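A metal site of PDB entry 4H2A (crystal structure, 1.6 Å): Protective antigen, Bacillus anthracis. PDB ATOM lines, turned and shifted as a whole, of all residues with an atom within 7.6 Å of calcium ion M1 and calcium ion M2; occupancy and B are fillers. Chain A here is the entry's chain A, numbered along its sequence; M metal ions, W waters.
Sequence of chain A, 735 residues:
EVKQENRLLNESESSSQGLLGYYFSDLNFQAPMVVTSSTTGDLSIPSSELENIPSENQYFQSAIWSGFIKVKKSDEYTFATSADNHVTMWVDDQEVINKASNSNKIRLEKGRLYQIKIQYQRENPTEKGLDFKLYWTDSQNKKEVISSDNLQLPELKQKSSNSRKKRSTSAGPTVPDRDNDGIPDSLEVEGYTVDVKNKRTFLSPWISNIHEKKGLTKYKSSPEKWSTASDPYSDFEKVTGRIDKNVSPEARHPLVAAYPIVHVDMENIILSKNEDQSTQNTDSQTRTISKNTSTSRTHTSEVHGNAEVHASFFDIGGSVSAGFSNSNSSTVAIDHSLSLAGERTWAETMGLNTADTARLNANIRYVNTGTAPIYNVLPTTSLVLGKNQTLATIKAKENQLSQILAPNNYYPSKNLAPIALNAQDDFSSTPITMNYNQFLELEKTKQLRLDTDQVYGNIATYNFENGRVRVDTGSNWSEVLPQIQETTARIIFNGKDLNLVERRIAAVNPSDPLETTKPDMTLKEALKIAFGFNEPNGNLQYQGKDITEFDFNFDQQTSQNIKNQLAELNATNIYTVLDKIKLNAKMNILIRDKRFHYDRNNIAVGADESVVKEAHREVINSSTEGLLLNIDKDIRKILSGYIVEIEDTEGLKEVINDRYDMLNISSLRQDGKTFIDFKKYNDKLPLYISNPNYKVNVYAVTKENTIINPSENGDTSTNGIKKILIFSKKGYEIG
Calcium ion M2 is bound by OD1 of Asp 177 (2.3 Å), OE1 of Glu 188 (2.3 Å), water W1 (2.3 Å), O of Ile 183 (2.4 Å), OD1 of Asp 181 (2.4 Å) and OD1 of Asp 179 (2.4 Å).
Calcium ion M2 has six donor atoms within binding distance.
Five residues have an atom within 4 Å of calcium ion M2: Asp 177, Asp 179, Asp 181, Ile 183 and Glu 188.
The nearest printed residue that does not touch calcium ion M2 is Gly 182 (4.4 Å).
Merely in contact with calcium ion M1: Thr 228 (3.98 Å).
Seven residues have an atom within 4 Å of calcium ion M1: Asp 179, Asp 181, Glu 188, Ser 222, Lys 225, Thr 228 and Asp 235.
Calcium ion M1 is bound by the backbone carbonyl oxygen (O) of Ser 222 (2.3 Å).
The side-chain carboxylate (OD2) of Asp 235 is bound to calcium ion M1 (2.3 Å).
Calcium ion M1 is bound by OD2 of Asp 181 (2.4 Å).
O of Lys 225 binds calcium ion M1 (2.4 Å).
The side-chain carboxylate (OE2) of Glu 188 binds calcium ion M1 (2.4 Å).
Calcium ion M1 is bound by the side-chain carboxylate (OD2) of Asp 179 (2.4 Å).
Calcium ion M1 is bound by the side-chain carboxylate (OE1) of Glu 188, 2.8 Å away.
The side-chain carboxylate of Asp 177 sits at hydrogen-bond distance from the backbone NH of Gly 182 (2.9 Å).
The backbone NH (N) of Lys 225 sits at hydrogen-bond distance from the side-chain hydroxyl (OG) of Ser 222.
The backbone NH of Ser 222 is in hydrogen-bond range of the side-chain hydroxyl of Thr 228.
N of Asp 179 lies close to O of Pro 223 (3.4 Å).
OG of Ser 222 lies within hydrogen-bond range of N of Glu 224 (3.0 Å).
The backbone carbonyl oxygen of Glu 188 is in hydrogen-bond range of the backbone NH of Ser 221, 3.0 Å away.
The backbone NH (N) of Thr 228 lies within hydrogen-bond range of the side-chain carboxylate (OD1) of Asp 235 (2.8 Å).
N of Asp 177 sits close to OD1 of Asp 185, 3.4 Å away.
Water W1 lies within hydrogen-bond range of the side-chain carboxylate of Asp 185 (2.5 Å), the backbone carbonyl oxygen of Pro 223 (2.9 Å) and the backbone NH of Arg 178 (3.4 Å).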
ATOM      1  N   PRO A 176     -19.817 -26.366  11.243  1.00  0.00           N
ATOM      2  CA  PRO A 176     -18.970 -25.292  11.717  1.00  0.00           C
ATOM      3  C   PRO A 176     -19.756 -23.986  11.733  1.00  0.00           C
ATOM      4  O   PRO A 176     -20.306 -23.595  10.730  1.00  0.00           O
ATOM      5  CB  PRO A 176     -17.832 -25.268  10.704  1.00  0.00           C
ATOM      6  CG  PRO A 176     -17.784 -26.696  10.202  1.00  0.00           C
ATOM      7  CD  PRO A 176     -19.232 -27.014  10.063  1.00  0.00           C
ATOM      8  N   ASP A 177     -19.816 -23.393  12.913  1.00  0.00           N
ATOM      9  CA  ASP A 177     -20.590 -22.165  13.166  1.00  0.00           C
ATOM     10  C   ASP A 177     -19.916 -21.492  14.367  1.00  0.00           C
ATOM     11  O   ASP A 177     -20.450 -21.488  15.492  1.00  0.00           O
ATOM     12  CB  ASP A 177     -22.038 -22.504  13.430  1.00  0.00           C
ATOM     13  CG  ASP A 177     -22.883 -21.274  13.709  1.00  0.00           C
ATOM     14  OD1 ASP A 177     -22.454 -20.201  13.267  1.00  0.00           O
ATOM     15  OD2 ASP A 177     -23.926 -21.390  14.341  1.00  0.00           O
ATOM     16  N   ARG A 178     -18.746 -20.928  14.111  1.00  0.00           N
ATOM     17  CA  ARG A 178     -17.854 -20.447  15.180  1.00  0.00           C
ATOM     18  C   ARG A 178     -18.546 -19.405  16.066  1.00  0.00           C
ATOM     19  O   ARG A 178     -18.403 -19.411  17.287  1.00  0.00           O
ATOM     20  CB  ARG A 178     -16.519 -19.882  14.633  1.00  0.00           C
ATOM     21  CG  ARG A 178     -15.557 -19.361  15.690  1.00  0.00           C
ATOM     22  CD  ARG A 178     -15.059 -20.462  16.623  1.00  0.00           C
ATOM     23  NE  ARG A 178     -14.062 -20.001  17.605  1.00  0.00           N
ATOM     24  CZ  ARG A 178     -14.333 -19.431  18.777  1.00  0.00           C
ATOM     25  NH1 ARG A 178     -15.583 -19.205  19.159  1.00  0.00           N
ATOM     26  NH2 ARG A 178     -13.339 -19.058  19.581  1.00  0.00           N
ATOM     27  N   ASP A 179     -19.321 -18.522  15.458  1.00  0.00           N
ATOM     28  CA  ASP A 179     -19.948 -17.473  16.233  1.00  0.00           C
ATOM     29  C   ASP A 179     -21.338 -17.801  16.774  1.00  0.00           C
ATOM     30  O   ASP A 179     -21.958 -16.974  17.450  1.00  0.00           O
ATOM     31  CB  ASP A 179     -19.991 -16.173  15.426  1.00  0.00           C
ATOM     32  CG  ASP A 179     -20.744 -16.317  14.108  1.00  0.00           C
ATOM     33  OD1 ASP A 179     -21.447 -17.332  13.905  1.00  0.00           O
ATOM     34  OD2 ASP A 179     -20.574 -15.418  13.287  1.00  0.00           O
ATOM     35  N   ASN A 180     -21.839 -19.020  16.527  1.00  0.00           N
ATOM     36  CA  ASN A 180     -23.129 -19.478  17.066  1.00  0.00           C
ATOM     37  C   ASN A 180     -24.344 -18.627  16.646  1.00  0.00           C
ATOM     38  O   ASN A 180     -25.344 -18.605  17.354  1.00  0.00           O
ATOM     39  CB  ASN A 180     -23.039 -19.601  18.614  1.00  0.00           C
ATOM     40  CG  ASN A 180     -23.998 -20.643  19.187  1.00  0.00           C
ATOM     41  OD1 ASN A 180     -24.015 -21.788  18.712  1.00  0.00           O
ATOM     42  ND2 ASN A 180     -24.801 -20.256  20.166  1.00  0.00           N
ATOM     43  N   ASP A 181     -24.298 -17.982  15.477  1.00  0.00           N
ATOM     44  CA  ASP A 181     -25.486 -17.288  14.974  1.00  0.00           C
ATOM     45  C   ASP A 181     -26.415 -18.213  14.232  1.00  0.00           C
ATOM     46  O   ASP A 181     -27.556 -17.873  14.009  1.00  0.00           O
ATOM     47  CB  ASP A 181     -25.169 -15.998  14.170  1.00  0.00           C
ATOM     48  CG  ASP A 181     -24.311 -16.200  12.951  1.00  0.00           C
ATOM     49  OD1 ASP A 181     -24.184 -17.347  12.414  1.00  0.00           O
ATOM     50  OD2 ASP A 181     -23.719 -15.193  12.476  1.00  0.00           O
ATOM     51  N   GLY A 182     -25.939 -19.404  13.881  1.00  0.00           N
ATOM     52  CA  GLY A 182     -26.795 -20.351  13.163  1.00  0.00           C
ATOM     53  C   GLY A 182     -26.439 -20.515  11.706  1.00  0.00           C
ATOM     54  O   GLY A 182     -26.887 -21.475  11.046  1.00  0.00           O
ATOM     55  N   ILE A 183     -25.687 -19.558  11.161  1.00  0.00           N
ATOM     56  CA  ILE A 183     -25.331 -19.599   9.731  1.00  0.00           C
ATOM     57  C   ILE A 183     -23.971 -20.282   9.625  1.00  0.00           C
ATOM     58  O   ILE A 183     -22.980 -19.826  10.195  1.00  0.00           O
ATOM     59  CB  ILE A 183     -25.251 -18.195   9.052  1.00  0.00           C
ATOM     60  CG1 ILE A 183     -26.448 -17.307   9.382  1.00  0.00           C
ATOM     61  CG2 ILE A 183     -25.112 -18.341   7.524  1.00  0.00           C
ATOM     62  CD1 ILE A 183     -26.358 -15.902   8.793  1.00  0.00           C
ATOM     63  N   PRO A 184     -23.894 -21.402   8.891  1.00  0.00           N
ATOM     64  CA  PRO A 184     -22.603 -22.066   8.784  1.00  0.00           C
ATOM     65  C   PRO A 184     -21.470 -21.161   8.299  1.00  0.00           C
ATOM     66  O   PRO A 184     -21.688 -20.326   7.401  1.00  0.00           O
ATOM     67  CB  PRO A 184     -22.872 -23.179   7.757  1.00  0.00           C
ATOM     68  CG  PRO A 184     -24.304 -23.471   7.867  1.00  0.00           C
ATOM     69  CD  PRO A 184     -24.962 -22.114   8.147  1.00  0.00           C
ATOM     70  N   ASP A 185     -20.264 -21.366   8.840  1.00  0.00           N
ATOM     71  CA  ASP A 185     -19.035 -20.644   8.454  1.00  0.00           C
ATOM     72  C   ASP A 185     -18.935 -20.456   6.942  1.00  0.00           C
ATOM     73  O   ASP A 185     -18.769 -19.335   6.446  1.00  0.00           O
ATOM     74  CB  ASP A 185     -17.760 -21.382   8.880  1.00  0.00           C
ATOM     75  CG  ASP A 185     -17.538 -21.426  10.390  1.00  0.00           C
ATOM     76  OD1 ASP A 185     -18.336 -20.889  11.179  1.00  0.00           O
ATOM     77  OD2 ASP A 185     -16.535 -22.052  10.770  1.00  0.00           O
ATOM     78  N   SER A 186     -19.036 -21.568   6.196  1.00  0.00           N
ATOM     79  CA  SER A 186     -18.846 -21.549   4.753  1.00  0.00           C
ATOM     80  C   SER A 186     -19.809 -20.635   4.020  1.00  0.00           C
ATOM     81  O   SER A 186     -19.417 -19.929   3.088  1.00  0.00           O
ATOM     82  CB  SER A 186     -18.932 -22.982   4.181  1.00  0.00           C
ATOM     83  OG  SER A 186     -20.243 -23.541   4.284  1.00  0.00           O
ATOM     84  N   GLU A 188     -21.426 -18.006   5.273  1.00  0.00           N
ATOM     85  CA  GLU A 188     -21.159 -16.581   5.587  1.00  0.00           C
ATOM     86  C   GLU A 188     -20.048 -16.018   4.722  1.00  0.00           C
ATOM     87  O   GLU A 188     -20.133 -14.900   4.236  1.00  0.00           O
ATOM     88  CB  GLU A 188     -20.841 -16.372   7.081  1.00  0.00           C
ATOM     89  CG  GLU A 188     -21.982 -16.707   8.008  1.00  0.00           C
ATOM     90  CD  GLU A 188     -21.887 -16.008   9.348  1.00  0.00           C
ATOM     91  OE1 GLU A 188     -21.656 -16.628  10.391  1.00  0.00           O
ATOM     92  OE2 GLU A 188     -22.055 -14.774   9.360  1.00  0.00           O
ATOM     93  N   TYR A 192     -24.654 -16.098   0.691  1.00  0.00           N
ATOM     94  CA  TYR A 192     -25.933 -16.778   0.861  1.00  0.00           C
ATOM     95  C   TYR A 192     -27.066 -15.841   0.544  1.00  0.00           C
ATOM     96  O   TYR A 192     -26.860 -14.626   0.389  1.00  0.00           O
ATOM     97  CB  TYR A 192     -26.066 -17.309   2.312  1.00  0.00           C
ATOM     98  CG  TYR A 192     -25.926 -16.249   3.430  1.00  0.00           C
ATOM     99  CD1 TYR A 192     -27.045 -15.702   4.063  1.00  0.00           C
ATOM    100  CD2 TYR A 192     -24.669 -15.828   3.853  1.00  0.00           C
ATOM    101  CE1 TYR A 192     -26.921 -14.736   5.071  1.00  0.00           C
ATOM    102  CE2 TYR A 192     -24.524 -14.901   4.887  1.00  0.00           C
ATOM    103  CZ  TYR A 192     -25.650 -14.366   5.493  1.00  0.00           C
ATOM    104  OH  TYR A 192     -25.464 -13.421   6.490  1.00  0.00           O
ATOM    105  N   SER A 221     -21.163 -12.250   5.303  1.00  0.00           N
ATOM    106  CA  SER A 221     -21.043 -11.824   6.705  1.00  0.00           C
ATOM    107  C   SER A 221     -19.836 -12.500   7.370  1.00  0.00           C
ATOM    108  O   SER A 221     -19.227 -13.416   6.771  1.00  0.00           O
ATOM    109  CB  SER A 221     -22.358 -12.065   7.454  1.00  0.00           C
ATOM    110  OG  SER A 221     -22.858 -13.382   7.317  1.00  0.00           O
ATOM    111  N   SER A 222     -19.408 -12.013   8.525  1.00  0.00           N
ATOM    112  CA  SER A 222     -18.283 -12.648   9.225  1.00  0.00           C
ATOM    113  C   SER A 222     -18.702 -13.905   9.980  1.00  0.00           C
ATOM    114  O   SER A 222     -19.653 -13.873  10.789  1.00  0.00           O
ATOM    115  CB  SER A 222     -17.659 -11.704  10.227  1.00  0.00           C
ATOM    116  OG  SER A 222     -16.717 -12.404  10.989  1.00  0.00           O
ATOM    117  N   PRO A 223     -17.999 -15.025   9.741  1.00  0.00           N
ATOM    118  CA  PRO A 223     -18.250 -16.227  10.513  1.00  0.00           C
ATOM    119  C   PRO A 223     -17.704 -16.179  11.931  1.00  0.00           C
ATOM    120  O   PRO A 223     -17.930 -17.095  12.733  1.00  0.00           O
ATOM    121  CB  PRO A 223     -17.558 -17.311   9.680  1.00  0.00           C
ATOM    122  CG  PRO A 223     -16.360 -16.601   9.120  1.00  0.00           C
ATOM    123  CD  PRO A 223     -16.897 -15.215   8.783  1.00  0.00           C
ATOM    124  N   GLU A 224     -16.985 -15.120  12.271  1.00  0.00           N
ATOM    125  CA  GLU A 224     -16.499 -14.910  13.615  1.00  0.00           C
ATOM    126  C   GLU A 224     -17.204 -13.813  14.406  1.00  0.00           C
ATOM    127  O   GLU A 224     -16.916 -13.652  15.597  1.00  0.00           O
ATOM    128  CB  GLU A 224     -15.001 -14.637  13.570  1.00  0.00           C
ATOM    129  CG  GLU A 224     -14.274 -15.753  12.832  1.00  0.00           C
ATOM    130  CD  GLU A 224     -12.893 -16.077  13.349  1.00  0.00           C
ATOM    131  OE1 GLU A 224     -12.637 -15.868  14.558  1.00  0.00           O
ATOM    132  OE2 GLU A 224     -12.066 -16.560  12.541  1.00  0.00           O
ATOM    133  N   LYS A 225     -18.167 -13.136  13.783  1.00  0.00           N
ATOM    134  CA  LYS A 225     -18.959 -12.117  14.474  1.00  0.00           C
ATOM    135  C   LYS A 225     -20.421 -12.513  14.404  1.00  0.00           C
ATOM    136  O   LYS A 225     -21.024 -12.614  13.333  1.00  0.00           O
ATOM    137  CB  LYS A 225     -18.753 -10.729  13.823  1.00  0.00           C
ATOM    138  CG  LYS A 225     -17.323 -10.172  13.923  1.00  0.00           C
ATOM    139  CD  LYS A 225     -17.143  -8.806  13.247  1.00  0.00           C
ATOM    140  CE  LYS A 225     -17.901  -7.636  13.907  1.00  0.00           C
ATOM    141  NZ  LYS A 225     -17.408  -7.235  15.237  1.00  0.00           N
ATOM    142  N   TRP A 226     -20.973 -12.781  15.580  1.00  0.00           N
ATOM    143  CA  TRP A 226     -22.380 -13.068  15.741  1.00  0.00           C
ATOM    144  C   TRP A 226     -23.256 -12.006  15.108  1.00  0.00           C
ATOM    145  O   TRP A 226     -24.242 -12.324  14.421  1.00  0.00           O
ATOM    146  CB  TRP A 226     -22.637 -13.259  17.233  1.00  0.00           C
ATOM    147  CG  TRP A 226     -24.044 -13.551  17.630  1.00  0.00           C
ATOM    148  CD1 TRP A 226     -24.656 -14.784  17.727  1.00  0.00           C
ATOM    149  CD2 TRP A 226     -25.030 -12.589  18.080  1.00  0.00           C
ATOM    150  NE1 TRP A 226     -25.945 -14.655  18.145  1.00  0.00           N
ATOM    151  CE2 TRP A 226     -26.238 -13.355  18.383  1.00  0.00           C
ATOM    152  CE3 TRP A 226     -25.060 -11.193  18.201  1.00  0.00           C
ATOM    153  CZ2 TRP A 226     -27.396 -12.743  18.832  1.00  0.00           C
ATOM    154  CZ3 TRP A 226     -26.232 -10.590  18.665  1.00  0.00           C
ATOM    155  CH2 TRP A 226     -27.376 -11.353  18.953  1.00  0.00           C
ATOM    156  N   SER A 227     -22.931 -10.733  15.347  1.00  0.00           N
ATOM    157  CA  SER A 227     -23.426  -9.597  14.567  1.00  0.00           C
ATOM    158  C   SER A 227     -22.282  -8.932  13.817  1.00  0.00           C
ATOM    159  O   SER A 227     -21.332  -8.332  14.432  1.00  0.00           O
ATOM    160  CB  SER A 227     -24.058  -8.548  15.470  1.00  0.00           C
ATOM    161  OG  SER A 227     -24.403  -7.425  14.713  1.00  0.00           O
ATOM    162  N   THR A 228     -22.286  -9.028  12.493  1.00  0.00           N
ATOM    163  CA  THR A 228     -21.160  -8.518  11.713  1.00  0.00           C
ATOM    164  C   THR A 228     -21.006  -7.001  11.789  1.00  0.00           C
ATOM    165  O   THR A 228     -19.903  -6.496  11.735  1.00  0.00           O
ATOM    166  CB  THR A 228     -21.210  -9.048  10.265  1.00  0.00           C
ATOM    167  OG1 THR A 228     -21.015 -10.460  10.312  1.00  0.00           O
ATOM    168  CG2 THR A 228     -20.090  -8.426   9.421  1.00  0.00           C
ATOM    169  N   SER A 234     -28.306 -10.679  15.642  1.00  0.00           N
ATOM    170  CA  SER A 234     -27.393 -11.570  14.936  1.00  0.00           C
ATOM    171  C   SER A 234     -27.613 -11.532  13.403  1.00  0.00           C
ATOM    172  O   SER A 234     -28.617 -11.094  12.901  1.00  0.00           O
ATOM    173  CB  SER A 234     -27.480 -13.023  15.404  1.00  0.00           C
ATOM    174  OG  SER A 234     -28.452 -13.736  14.631  1.00  0.00           O
ATOM    175  N   ASP A 235     -26.608 -11.979  12.696  1.00  0.00           N
ATOM    176  CA  ASP A 235     -26.659 -12.033  11.232  1.00  0.00           C
ATOM    177  C   ASP A 235     -27.868 -12.910  10.800  1.00  0.00           C
ATOM    178  O   ASP A 235     -28.519 -12.602   9.821  1.00  0.00           O
ATOM    179  CB  ASP A 235     -25.348 -12.612  10.747  1.00  0.00           C
ATOM    180  CG  ASP A 235     -24.135 -11.716  11.003  1.00  0.00           C
ATOM    181  OD1 ASP A 235     -24.289 -10.486  11.159  1.00  0.00           O
ATOM    182  OD2 ASP A 235     -23.024 -12.257  11.017  1.00  0.00           O
ATOM    183  N   PHE A 236     -28.124 -13.983  11.546  1.00  0.00           N
ATOM    184  CA  PHE A 236     -29.225 -14.931  11.281  1.00  0.00           C
ATOM    185  C   PHE A 236     -30.545 -14.340  11.660  1.00  0.00           C
ATOM    186  O   PHE A 236     -31.545 -14.467  10.952  1.00  0.00           O
ATOM    187  CB  PHE A 236     -28.971 -16.231  12.035  1.00  0.00           C
ATOM    188  CG  PHE A 236     -30.008 -17.294  11.838  1.00  0.00           C
ATOM    189  CD1 PHE A 236     -30.068 -18.036  10.667  1.00  0.00           C
ATOM    190  CD2 PHE A 236     -30.887 -17.607  12.883  1.00  0.00           C
ATOM    191  CE1 PHE A 236     -31.039 -19.023  10.510  1.00  0.00           C
ATOM    192  CE2 PHE A 236     -31.846 -18.599  12.728  1.00  0.00           C
ATOM    193  CZ  PHE A 236     -31.894 -19.310  11.548  1.00  0.00           C
ATOM    194  N   PRO A 254     -26.901  -7.921   7.186  1.00  0.00           N
ATOM    195  CA  PRO A 254     -25.870  -8.102   8.185  1.00  0.00           C
ATOM    196  C   PRO A 254     -24.740  -7.082   8.177  1.00  0.00           C
ATOM    197  O   PRO A 254     -24.020  -7.005   9.164  1.00  0.00           O
ATOM    198  CB  PRO A 254     -25.324  -9.530   7.886  1.00  0.00           C
ATOM    199  CG  PRO A 254     -26.488 -10.201   7.270  1.00  0.00           C
ATOM    200  CD  PRO A 254     -27.173  -9.161   6.432  1.00  0.00           C
HETATM  201 CA    CA M   1     -21.776 -14.129  11.647  1.00  0.00          CA
HETATM  202 CA    CA M   2     -22.114 -18.384  11.866  1.00  0.00          CA
HETATM  203  O   HOH W   1     -19.840 -18.923  11.643  1.00  0.00           O
